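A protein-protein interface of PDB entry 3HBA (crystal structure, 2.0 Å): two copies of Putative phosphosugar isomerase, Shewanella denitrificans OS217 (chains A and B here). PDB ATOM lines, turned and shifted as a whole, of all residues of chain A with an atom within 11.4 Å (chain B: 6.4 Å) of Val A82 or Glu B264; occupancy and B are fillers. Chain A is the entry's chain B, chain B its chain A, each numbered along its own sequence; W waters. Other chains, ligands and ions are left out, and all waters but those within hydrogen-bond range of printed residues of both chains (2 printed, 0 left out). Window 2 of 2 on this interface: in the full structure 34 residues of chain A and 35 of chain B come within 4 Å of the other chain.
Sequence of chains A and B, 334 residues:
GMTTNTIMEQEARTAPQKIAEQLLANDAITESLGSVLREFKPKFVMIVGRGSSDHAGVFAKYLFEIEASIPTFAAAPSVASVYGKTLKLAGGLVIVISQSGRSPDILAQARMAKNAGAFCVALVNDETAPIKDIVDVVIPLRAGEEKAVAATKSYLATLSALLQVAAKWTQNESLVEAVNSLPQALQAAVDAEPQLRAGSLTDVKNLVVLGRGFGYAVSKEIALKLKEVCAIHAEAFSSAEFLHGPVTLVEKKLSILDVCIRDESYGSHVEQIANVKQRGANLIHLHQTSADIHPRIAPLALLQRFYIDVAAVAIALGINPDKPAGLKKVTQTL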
ATOM      1  N   ALA A  75     -24.747  21.850  24.198  1.00  0.00           N
ATOM      2  CA  ALA A  75     -23.444  21.578  23.684  1.00  0.00           C
ATOM      3  C   ALA A  75     -23.545  21.402  22.159  1.00  0.00           C
ATOM      4  O   ALA A  75     -24.558  20.942  21.655  1.00  0.00           O
ATOM      5  CB  ALA A  75     -22.906  20.313  24.341  1.00  0.00           C
ATOM      6  N   ALA A  76     -22.487  21.778  21.448  1.00  0.00           N
ATOM      7  CA  ALA A  76     -22.298  21.510  20.014  1.00  0.00           C
ATOM      8  C   ALA A  76     -21.360  20.307  19.857  1.00  0.00           C
ATOM      9  O   ALA A  76     -20.136  20.410  20.079  1.00  0.00           O
ATOM     10  CB  ALA A  76     -21.725  22.802  19.257  1.00  0.00           C
ATOM     11  N   PRO A  77     -21.901  19.136  19.491  1.00  0.00           N
ATOM     12  CA  PRO A  77     -21.046  17.961  19.496  1.00  0.00           C
ATOM     13  C   PRO A  77     -19.764  18.078  18.682  1.00  0.00           C
ATOM     14  O   PRO A  77     -18.742  17.549  19.089  1.00  0.00           O
ATOM     15  CB  PRO A  77     -21.962  16.875  18.900  1.00  0.00           C
ATOM     16  CG  PRO A  77     -23.288  17.247  19.385  1.00  0.00           C
ATOM     17  CD  PRO A  77     -23.300  18.762  19.241  1.00  0.00           C
ATOM     18  N   SER A  78     -19.815  18.744  17.537  1.00  0.00           N
ATOM     19  CA  SER A  78     -18.650  18.837  16.677  1.00  0.00           C
ATOM     20  C   SER A  78     -17.450  19.500  17.357  1.00  0.00           C
ATOM     21  O   SER A  78     -16.284  19.230  16.986  1.00  0.00           O
ATOM     22  CB  SER A  78     -18.989  19.588  15.396  1.00  0.00           C
ATOM     23  OG  SER A  78     -19.424  20.915  15.683  1.00  0.00           O
ATOM     24  N   VAL A  79     -17.710  20.423  18.281  1.00  0.00           N
ATOM     25  CA  VAL A  79     -16.596  21.139  18.952  1.00  0.00           C
ATOM     26  C   VAL A  79     -15.639  20.116  19.607  1.00  0.00           C
ATOM     27  O   VAL A  79     -14.427  20.228  19.523  1.00  0.00           O
ATOM     28  CB  VAL A  79     -17.134  22.164  20.013  1.00  0.00           C
ATOM     29  CG1 VAL A  79     -16.019  22.651  20.860  1.00  0.00           C
ATOM     30  CG2 VAL A  79     -17.813  23.314  19.325  1.00  0.00           C
ATOM     31  N   ALA A  80     -16.237  19.105  20.224  1.00  0.00           N
ATOM     32  CA  ALA A  80     -15.536  18.016  20.897  1.00  0.00           C
ATOM     33  C   ALA A  80     -15.121  16.937  19.907  1.00  0.00           C
ATOM     34  O   ALA A  80     -13.992  16.536  19.923  1.00  0.00           O
ATOM     35  CB  ALA A  80     -16.411  17.409  21.980  1.00  0.00           C
ATOM     36  N   SER A  81     -16.013  16.507  19.019  1.00  0.00           N
ATOM     37  CA  SER A  81     -15.695  15.367  18.132  1.00  0.00           C
ATOM     38  C   SER A  81     -14.828  15.734  16.938  1.00  0.00           C
ATOM     39  O   SER A  81     -13.829  15.114  16.712  1.00  0.00           O
ATOM     40  CB  SER A  81     -16.963  14.715  17.624  1.00  0.00           C
ATOM     41  OG  SER A  81     -17.620  15.586  16.715  1.00  0.00           O
ATOM     42  N   VAL A  82     -15.218  16.739  16.180  1.00  0.00           N
ATOM     43  CA  VAL A  82     -14.515  17.131  14.962  1.00  0.00           C
ATOM     44  C   VAL A  82     -13.369  18.117  15.217  1.00  0.00           C
ATOM     45  O   VAL A  82     -12.282  18.000  14.656  1.00  0.00           O
ATOM     46  CB  VAL A  82     -15.561  17.748  13.975  1.00  0.00           C
ATOM     47  CG1 VAL A  82     -14.922  18.711  12.996  1.00  0.00           C
ATOM     48  CG2 VAL A  82     -16.287  16.621  13.241  1.00  0.00           C
ATOM     49  N   TYR A  83     -13.598  19.108  16.069  1.00  0.00           N
ATOM     50  CA  TYR A  83     -12.556  20.120  16.285  1.00  0.00           C
ATOM     51  C   TYR A  83     -11.619  19.723  17.437  1.00  0.00           C
ATOM     52  O   TYR A  83     -10.602  20.375  17.641  1.00  0.00           O
ATOM     53  CB  TYR A  83     -13.173  21.517  16.472  1.00  0.00           C
ATOM     54  CG  TYR A  83     -13.844  22.026  15.216  1.00  0.00           C
ATOM     55  CD1 TYR A  83     -13.140  22.718  14.253  1.00  0.00           C
ATOM     56  CD2 TYR A  83     -15.186  21.783  14.989  1.00  0.00           C
ATOM     57  CE1 TYR A  83     -13.773  23.190  13.111  1.00  0.00           C
ATOM     58  CE2 TYR A  83     -15.831  22.255  13.845  1.00  0.00           C
ATOM     59  CZ  TYR A  83     -15.149  22.947  12.928  1.00  0.00           C
ATOM     60  OH  TYR A  83     -15.799  23.382  11.763  1.00  0.00           O
ATOM     61  N   GLY A  84     -11.953  18.642  18.143  1.00  0.00           N
ATOM     62  CA  GLY A  84     -11.062  18.056  19.154  1.00  0.00           C
ATOM     63  C   GLY A  84     -10.823  18.919  20.385  1.00  0.00           C
ATOM     64  O   GLY A  84      -9.792  18.805  21.030  1.00  0.00           O
ATOM     65  N   LYS A  85     -11.780  19.775  20.725  1.00  0.00           N
ATOM     66  CA  LYS A  85     -11.571  20.735  21.808  1.00  0.00           C
ATOM     67  C   LYS A  85     -12.186  20.264  23.098  1.00  0.00           C
ATOM     68  O   LYS A  85     -13.250  19.630  23.086  1.00  0.00           O
ATOM     69  CB  LYS A  85     -12.138  22.124  21.406  1.00  0.00           C
ATOM     70  CG  LYS A  85     -11.428  22.762  20.176  1.00  0.00           C
ATOM     71  CD  LYS A  85      -9.907  22.996  20.297  1.00  0.00           C
ATOM     72  CE  LYS A  85      -9.287  23.427  18.935  1.00  0.00           C
ATOM     73  NZ  LYS A  85      -7.813  23.571  18.846  1.00  0.00           N
ATOM     74  N   THR A  86     -11.505  20.523  24.214  1.00  0.00           N
ATOM     75  CA  THR A  86     -12.075  20.316  25.560  1.00  0.00           C
ATOM     76  C   THR A  86     -12.397  21.704  26.167  1.00  0.00           C
ATOM     77  O   THR A  86     -11.516  22.544  26.268  1.00  0.00           O
ATOM     78  CB  THR A  86     -11.098  19.593  26.524  1.00  0.00           C
ATOM     79  OG1 THR A  86     -10.820  18.261  26.060  1.00  0.00           O
ATOM     80  CG2 THR A  86     -11.705  19.482  27.930  1.00  0.00           C
ATOM     81  N   PRO A 104     -21.681   6.223  21.210  1.00  0.00           N
ATOM     82  CA  PRO A 104     -20.269   6.554  21.436  1.00  0.00           C
ATOM     83  C   PRO A 104     -19.978   8.044  21.525  1.00  0.00           C
ATOM     84  O   PRO A 104     -19.099   8.474  22.284  1.00  0.00           O
ATOM     85  CB  PRO A 104     -19.572   5.938  20.220  1.00  0.00           C
ATOM     86  CG  PRO A 104     -20.416   4.791  19.858  1.00  0.00           C
ATOM     87  CD  PRO A 104     -21.832   5.204  20.156  1.00  0.00           C
ATOM     88  N   ASP A 105     -20.708   8.821  20.742  1.00  0.00           N
ATOM     89  CA  ASP A 105     -20.585  10.257  20.774  1.00  0.00           C
ATOM     90  C   ASP A 105     -21.055  10.838  22.128  1.00  0.00           C
ATOM     91  O   ASP A 105     -20.389  11.720  22.689  1.00  0.00           O
ATOM     92  CB  ASP A 105     -21.428  10.863  19.657  1.00  0.00           C
ATOM     93  CG  ASP A 105     -21.359  12.382  19.642  1.00  0.00           C
ATOM     94  OD1 ASP A 105     -20.237  12.916  19.450  1.00  0.00           O
ATOM     95  OD2 ASP A 105     -22.427  13.029  19.820  1.00  0.00           O
ATOM     96  N   ALA A 108     -18.487   9.965  24.655  1.00  0.00           N
ATOM     97  CA  ALA A 108     -17.295  10.805  24.475  1.00  0.00           C
ATOM     98  C   ALA A 108     -17.515  12.218  25.075  1.00  0.00           C
ATOM     99  O   ALA A 108     -16.661  12.748  25.821  1.00  0.00           O
ATOM    100  CB  ALA A 108     -16.922  10.891  22.984  1.00  0.00           C
ATOM    101  N   GLN A 109     -18.652  12.820  24.773  1.00  0.00           N
ATOM    102  CA  GLN A 109     -18.961  14.162  25.316  1.00  0.00           C
ATOM    103  C   GLN A 109     -18.995  14.146  26.855  1.00  0.00           C
ATOM    104  O   GLN A 109     -18.524  15.083  27.522  1.00  0.00           O
ATOM    105  CB  GLN A 109     -20.281  14.704  24.745  1.00  0.00           C
ATOM    106  CG  GLN A 109     -20.313  14.983  23.228  1.00  0.00           C
ATOM    107  CD  GLN A 109     -21.607  15.682  22.772  1.00  0.00           C
ATOM    108  OE1 GLN A 109     -21.902  16.817  23.172  1.00  0.00           O
ATOM    109  NE2 GLN A 109     -22.390  14.996  21.941  1.00  0.00           N
ATOM    110  N   MET A 112     -15.474  13.996  28.201  1.00  0.00           N
ATOM    111  CA  MET A 112     -14.875  15.352  28.035  1.00  0.00           C
ATOM    112  C   MET A 112     -15.387  16.282  29.165  1.00  0.00           C
ATOM    113  O   MET A 112     -14.580  16.948  29.839  1.00  0.00           O
ATOM    114  CB  MET A 112     -15.149  15.922  26.615  1.00  0.00           C
ATOM    115  CG  MET A 112     -14.625  17.399  26.275  1.00  0.00           C
ATOM    116  SD  MET A 112     -15.824  18.954  26.722  1.00  0.00           S
ATOM    117  CE  MET A 112     -16.512  19.479  24.972  1.00  0.00           C
ATOM    118  N   ILE B  66     -14.062  27.015  20.111  1.00  0.00           N
ATOM    119  CA  ILE B  66     -12.942  26.360  19.477  1.00  0.00           C
ATOM    120  C   ILE B  66     -11.608  27.099  19.698  1.00  0.00           C
ATOM    121  O   ILE B  66     -10.596  26.452  19.956  1.00  0.00           O
ATOM    122  CB  ILE B  66     -13.186  26.090  17.960  1.00  0.00           C
ATOM    123  CG1 ILE B  66     -14.293  25.030  17.748  1.00  0.00           C
ATOM    124  CG2 ILE B  66     -11.882  25.640  17.315  1.00  0.00           C
ATOM    125  CD1 ILE B  66     -15.000  25.138  16.361  1.00  0.00           C
ATOM    126  N   GLU B  67     -11.605  28.427  19.612  1.00  0.00           N
ATOM    127  CA  GLU B  67     -10.360  29.208  19.778  1.00  0.00           C
ATOM    128  C   GLU B  67     -10.020  29.510  21.229  1.00  0.00           C
ATOM    129  O   GLU B  67      -8.858  29.512  21.588  1.00  0.00           O
ATOM    130  CB  GLU B  67     -10.430  30.488  18.978  1.00  0.00           C
ATOM    131  CG  GLU B  67     -10.512  30.244  17.480  1.00  0.00           C
ATOM    132  CD  GLU B  67      -9.229  29.667  16.884  1.00  0.00           C
ATOM    133  OE1 GLU B  67      -8.138  29.945  17.451  1.00  0.00           O
ATOM    134  OE2 GLU B  67      -9.293  28.972  15.835  1.00  0.00           O
ATOM    135  N   ARG B 212     -21.252  21.384   8.316  1.00  0.00           N
ATOM    136  CA  ARG B 212     -20.753  20.865   9.583  1.00  0.00           C
ATOM    137  C   ARG B 212     -19.943  21.951  10.255  1.00  0.00           C
ATOM    138  O   ARG B 212     -19.239  22.683   9.567  1.00  0.00           O
ATOM    139  CB  ARG B 212     -19.883  19.635   9.291  1.00  0.00           C
ATOM    140  CG  ARG B 212     -19.573  18.800  10.487  1.00  0.00           C
ATOM    141  CD  ARG B 212     -20.720  17.867  10.804  1.00  0.00           C
ATOM    142  NE  ARG B 212     -20.688  17.449  12.204  1.00  0.00           N
ATOM    143  CZ  ARG B 212     -20.059  16.371  12.666  1.00  0.00           C
ATOM    144  NH1 ARG B 212     -19.365  15.573  11.875  1.00  0.00           N
ATOM    145  NH2 ARG B 212     -20.115  16.088  13.944  1.00  0.00           N
ATOM    146  N   GLY B 213     -20.047  22.099  11.581  1.00  0.00           N
ATOM    147  CA  GLY B 213     -19.228  23.058  12.325  1.00  0.00           C
ATOM    148  C   GLY B 213     -19.448  24.498  11.866  1.00  0.00           C
ATOM    149  O   GLY B 213     -20.579  24.945  11.747  1.00  0.00           O
ATOM    150  N   PHE B 214     -18.374  25.216  11.553  1.00  0.00           N
ATOM    151  CA  PHE B 214     -18.503  26.561  11.006  1.00  0.00           C
ATOM    152  C   PHE B 214     -19.372  26.527   9.727  1.00  0.00           C
ATOM    153  O   PHE B 214     -20.171  27.427   9.484  1.00  0.00           O
ATOM    154  CB  PHE B 214     -17.113  27.155  10.719  1.00  0.00           C
ATOM    155  CG  PHE B 214     -16.387  27.632  11.954  1.00  0.00           C
ATOM    156  CD1 PHE B 214     -16.698  28.858  12.525  1.00  0.00           C
ATOM    157  CD2 PHE B 214     -15.359  26.891  12.508  1.00  0.00           C
ATOM    158  CE1 PHE B 214     -16.018  29.326  13.632  1.00  0.00           C
ATOM    159  CE2 PHE B 214     -14.681  27.347  13.646  1.00  0.00           C
ATOM    160  CZ  PHE B 214     -15.015  28.593  14.192  1.00  0.00           C
ATOM    161  N   ILE B 261     -16.702  23.549   3.638  1.00  0.00           N
ATOM    162  CA  ILE B 261     -15.566  24.213   4.268  1.00  0.00           C
ATOM    163  C   ILE B 261     -14.409  23.264   4.499  1.00  0.00           C
ATOM    164  O   ILE B 261     -14.604  22.164   5.028  1.00  0.00           O
ATOM    165  CB  ILE B 261     -15.961  24.793   5.643  1.00  0.00           C
ATOM    166  CG1 ILE B 261     -17.150  25.739   5.471  1.00  0.00           C
ATOM    167  CG2 ILE B 261     -14.716  25.419   6.338  1.00  0.00           C
ATOM    168  CD1 ILE B 261     -16.898  26.822   4.446  1.00  0.00           C
ATOM    169  N   ARG B 262     -13.207  23.707   4.116  1.00  0.00           N
ATOM    170  CA  ARG B 262     -11.974  22.945   4.288  1.00  0.00           C
ATOM    171  C   ARG B 262     -11.337  23.276   5.650  1.00  0.00           C
ATOM    172  O   ARG B 262     -10.340  24.005   5.724  1.00  0.00           O
ATOM    173  CB  ARG B 262     -10.991  23.257   3.139  1.00  0.00           C
ATOM    174  CG  ARG B 262     -11.526  22.887   1.765  1.00  0.00           C
ATOM    175  CD  ARG B 262     -10.566  23.329   0.643  1.00  0.00           C
ATOM    176  NE  ARG B 262      -9.274  22.625   0.651  1.00  0.00           N
ATOM    177  CZ  ARG B 262      -9.081  21.371   0.235  1.00  0.00           C
ATOM    178  NH1 ARG B 262     -10.095  20.654  -0.224  1.00  0.00           N
ATOM    179  NH2 ARG B 262      -7.858  20.831   0.269  1.00  0.00           N
ATOM    180  N   ASP B 263     -11.947  22.781   6.731  1.00  0.00           N
ATOM    181  CA  ASP B 263     -11.376  22.904   8.060  1.00  0.00           C
ATOM    182  C   ASP B 263     -11.377  21.523   8.691  1.00  0.00           C
ATOM    183  O   ASP B 263     -11.475  20.545   7.990  1.00  0.00           O
ATOM    184  CB  ASP B 263     -12.105  23.953   8.916  1.00  0.00           C
ATOM    185  CG  ASP B 263     -13.568  23.600   9.223  1.00  0.00           C
ATOM    186  OD1 ASP B 263     -14.084  22.564   8.741  1.00  0.00           O
ATOM    187  OD2 ASP B 263     -14.207  24.400   9.949  1.00  0.00           O
ATOM    188  N   GLU B 264     -11.300  21.429  10.011  1.00  0.00           N
ATOM    189  CA  GLU B 264     -11.272  20.147  10.639  1.00  0.00           C
ATOM    190  C   GLU B 264     -12.534  19.303  10.343  1.00  0.00           C
ATOM    191  O   GLU B 264     -12.504  18.066  10.476  1.00  0.00           O
ATOM    192  CB  GLU B 264     -11.049  20.295  12.144  1.00  0.00           C
ATOM    193  CG  GLU B 264      -9.802  21.109  12.565  1.00  0.00           C
ATOM    194  CD  GLU B 264     -10.021  22.621  12.668  1.00  0.00           C
ATOM    195  OE1 GLU B 264     -10.568  23.270  11.733  1.00  0.00           O
ATOM    196  OE2 GLU B 264      -9.594  23.174  13.694  1.00  0.00           O
ATOM    197  N   SER B 265     -13.626  19.962   9.958  1.00  0.00           N
ATOM    198  CA  SER B 265     -14.896  19.275   9.704  1.00  0.00           C
ATOM    199  C   SER B 265     -14.965  18.640   8.318  1.00  0.00           C
ATOM    200  O   SER B 265     -15.880  17.870   8.049  1.00  0.00           O
ATOM    201  CB  SER B 265     -16.077  20.260   9.871  1.00  0.00           C
ATOM    202  OG  SER B 265     -16.259  21.098   8.726  1.00  0.00           O
ATOM    203  N   TYR B 266     -14.006  18.949   7.450  1.00  0.00           N
ATOM    204  CA  TYR B 266     -14.099  18.582   6.033  1.00  0.00           C
ATOM    205  C   TYR B 266     -14.283  17.089   5.815  1.00  0.00           C
ATOM    206  O   TYR B 266     -15.132  16.671   5.028  1.00  0.00           O
ATOM    207  CB  TYR B 266     -12.839  19.026   5.306  1.00  0.00           C
ATOM    208  CG  TYR B 266     -12.759  18.632   3.849  1.00  0.00           C
ATOM    209  CD1 TYR B 266     -13.283  19.451   2.856  1.00  0.00           C
ATOM    210  CD2 TYR B 266     -12.113  17.471   3.456  1.00  0.00           C
ATOM    211  CE1 TYR B 266     -13.207  19.094   1.522  1.00  0.00           C
ATOM    212  CE2 TYR B 266     -12.033  17.115   2.117  1.00  0.00           C
ATOM    213  CZ  TYR B 266     -12.574  17.930   1.161  1.00  0.00           C
ATOM    214  OH  TYR B 266     -12.485  17.579  -0.176  1.00  0.00           O
ATOM    215  N   GLY B 267     -13.498  16.303   6.535  1.00  0.00           N
ATOM    216  CA  GLY B 267     -13.473  14.847   6.359  1.00  0.00           C
ATOM    217  C   GLY B 267     -14.797  14.188   6.674  1.00  0.00           C
ATOM    218  O   GLY B 267     -15.326  13.426   5.855  1.00  0.00           O
ATOM    219  N   SER B 268     -15.347  14.488   7.856  1.00  0.00           N
ATOM    220  CA  SER B 268     -16.634  13.927   8.230  1.00  0.00           C
ATOM    221  C   SER B 268     -17.750  14.461   7.315  1.00  0.00           C
ATOM    222  O   SER B 268     -18.619  13.719   6.891  1.00  0.00           O
ATOM    223  CB  SER B 268     -16.942  14.170   9.714  1.00  0.00           C
ATOM    224  OG  SER B 268     -17.007  15.551   9.982  1.00  0.00           O
ATOM    225  N   PRO B 295      -8.501  28.239   7.443  1.00  0.00           N
ATOM    226  CA  PRO B 295      -9.773  27.602   7.735  1.00  0.00           C
ATOM    227  C   PRO B 295     -10.785  28.457   8.482  1.00  0.00           C
ATOM    228  O   PRO B 295     -12.005  28.262   8.289  1.00  0.00           O
ATOM    229  CB  PRO B 295      -9.368  26.376   8.580  1.00  0.00           C
ATOM    230  CG  PRO B 295      -7.949  26.581   8.900  1.00  0.00           C
ATOM    231  CD  PRO B 295      -7.381  27.364   7.803  1.00  0.00           C
ATOM    232  N   ARG B 296     -10.302  29.365   9.330  1.00  0.00           N
ATOM    233  CA  ARG B 296     -11.207  30.222  10.117  1.00  0.00           C
ATOM    234  C   ARG B 296     -11.782  31.364   9.289  1.00  0.00           C
ATOM    235  O   ARG B 296     -12.810  31.916   9.670  1.00  0.00           O
ATOM    236  CB  ARG B 296     -10.532  30.735  11.366  1.00  0.00           C
ATOM    237  CG  ARG B 296     -10.183  29.650  12.370  1.00  0.00           C
ATOM    238  CD  ARG B 296     -11.409  28.897  12.954  1.00  0.00           C
ATOM    239  NE  ARG B 296     -10.842  27.882  13.819  1.00  0.00           N
ATOM    240  CZ  ARG B 296     -10.640  26.617  13.493  1.00  0.00           C
ATOM    241  NH1 ARG B 296     -11.094  26.106  12.339  1.00  0.00           N
ATOM    242  NH2 ARG B 296      -9.996  25.845  14.358  1.00  0.00           N
HETATM  243  O   HOH W   1      -8.589  21.938  15.555  1.00  0.00           O
HETATM  244  O   HOH W   2     -16.793  24.004   9.018  1.00  0.00           O
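OD2 of Asp B263 sits at hydrogen-bond distance from OH of Tyr A83 (2.6 Å). OH of Tyr A83 is in hydrogen-bond range of N of Phe B214.
The side-chain hydroxyl (OG) of Ser B265 sits at hydrogen-bond distance from the side-chain carboxylate (OD1) of Asp B263 (2.6 Å). OG of Ser A81 lies within hydrogen-bond range of O of Pro A77. OG of Ser B268 is in hydrogen-bond range of O of Ser B265 (3.2 Å). The side-chain carboxylate (OE2) of Glu B264 is in salt-bridge range of the guanidinium group (NH2) of Arg B296. N of Lys A85 sits at hydrogen-bond distance from O of Val A79 (2.9 Å). O of Arg B212 lies within hydrogen-bond range of OG of Ser B265, at 3.5 Å.
Arg B212 touches Ser A78. OG of Ser A81 touches NH2 of Arg B212 (3.8 Å). Val A82 touches Arg B212. Glu B264 touches Val A82 (O to CG1, 3.6 Å). Ser B265 touches Val A82 (CA to CG1, 3.3 Å). Val A82 touches Ser B268. Tyr A83 touches Ile B66. Gly B213 touches Tyr A83 (CA to OH, 3.5 Å). Glu B264 touches Tyr A83 (OE1 to CE1, 3.5 Å). Ser B265 touches Tyr A83 (CB to OH, 3.7 Å).
Pro A77 touches none of the printed residues of chain B. Printed residues of chain B within 4 Å of Ser A78: Arg B212 and Gly B213. Val A82 touches just these residues of chain B: Arg B212 (3.5 Å), Glu B264 (3.6 Å), Ser B265 (3.3 Å) and Ser B268 (3.5 Å). Of the printed residues of chain B, Tyr A83 touches Ile B66 (3.5 Å), Gly B213 (3.5 Å), Phe B214 (3.2 Å), Asp B263 (2.6 Å), Glu B264 (3.5 Å) and Ser B265 (3.7 Å). Printed residues of chain B within 4 Å of Lys A85: Ile B66. Printed residues of chain A within 4 Å of Gly B213: Ser A78 (3.99 Å) and Tyr A83 (3.5 Å). Glu B264 touches just these residues of chain A: Val A82 (3.6 Å) and Tyr A83 (3.5 Å). Ser B265 touches two residues of chain A. No residue of chain A comes within 4 Å of Gly B267. No residue of chain A comes within 4 Å of Pro B295. The nearest residue of chain B that does not touch Val A82 is Tyr B266 (5.6 Å). The nearest residue of chain A that does not touch Glu B264 is Lys A85 (5.3 Å).
Of the 15 printed residues of chain B, 8 touch a printed residue of chain A. Printed residues of chain B that touch a printed residue of chain A: Ile B66, Arg B212, Gly B213, Phe B214, Asp B263, Glu B264, Ser B265 and Ser B268. Hydrophobic or aromatic side chains of chain B within 4 Å of the printed part of chain A: Ile B66 and Phe B214. Of the 17 printed residues of chain A, 5 touch a printed residue of chain B. Hydrophobic or aromatic side chains of chain A that line the printed part of chain B: Val A82 and Tyr A83. Along chain A the printed residues that touch a printed residue of chain B span positions 78 to 85. Among the printed residues, no Asp or Glu carboxylate lies within 4 Å of a Lys or Arg side-chain nitrogen of the other chain.
No position is printed for both chains. Of the 14 pairs that touch across the chains among the printed residues, none has its exchanged pair printed and touching as well.
Water W1 bridges OE2 of Glu B264 (2.4 Å) and O of Tyr A83 (3.3 Å). Water W2 lies within hydrogen-bond range of the side-chain carboxylate of Asp B263, the backbone carbonyl oxygen of Arg B212, the side-chain hydroxyl of Ser B265, the side-chain hydroxyl of Tyr A83 and the backbone NH of Phe B214.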
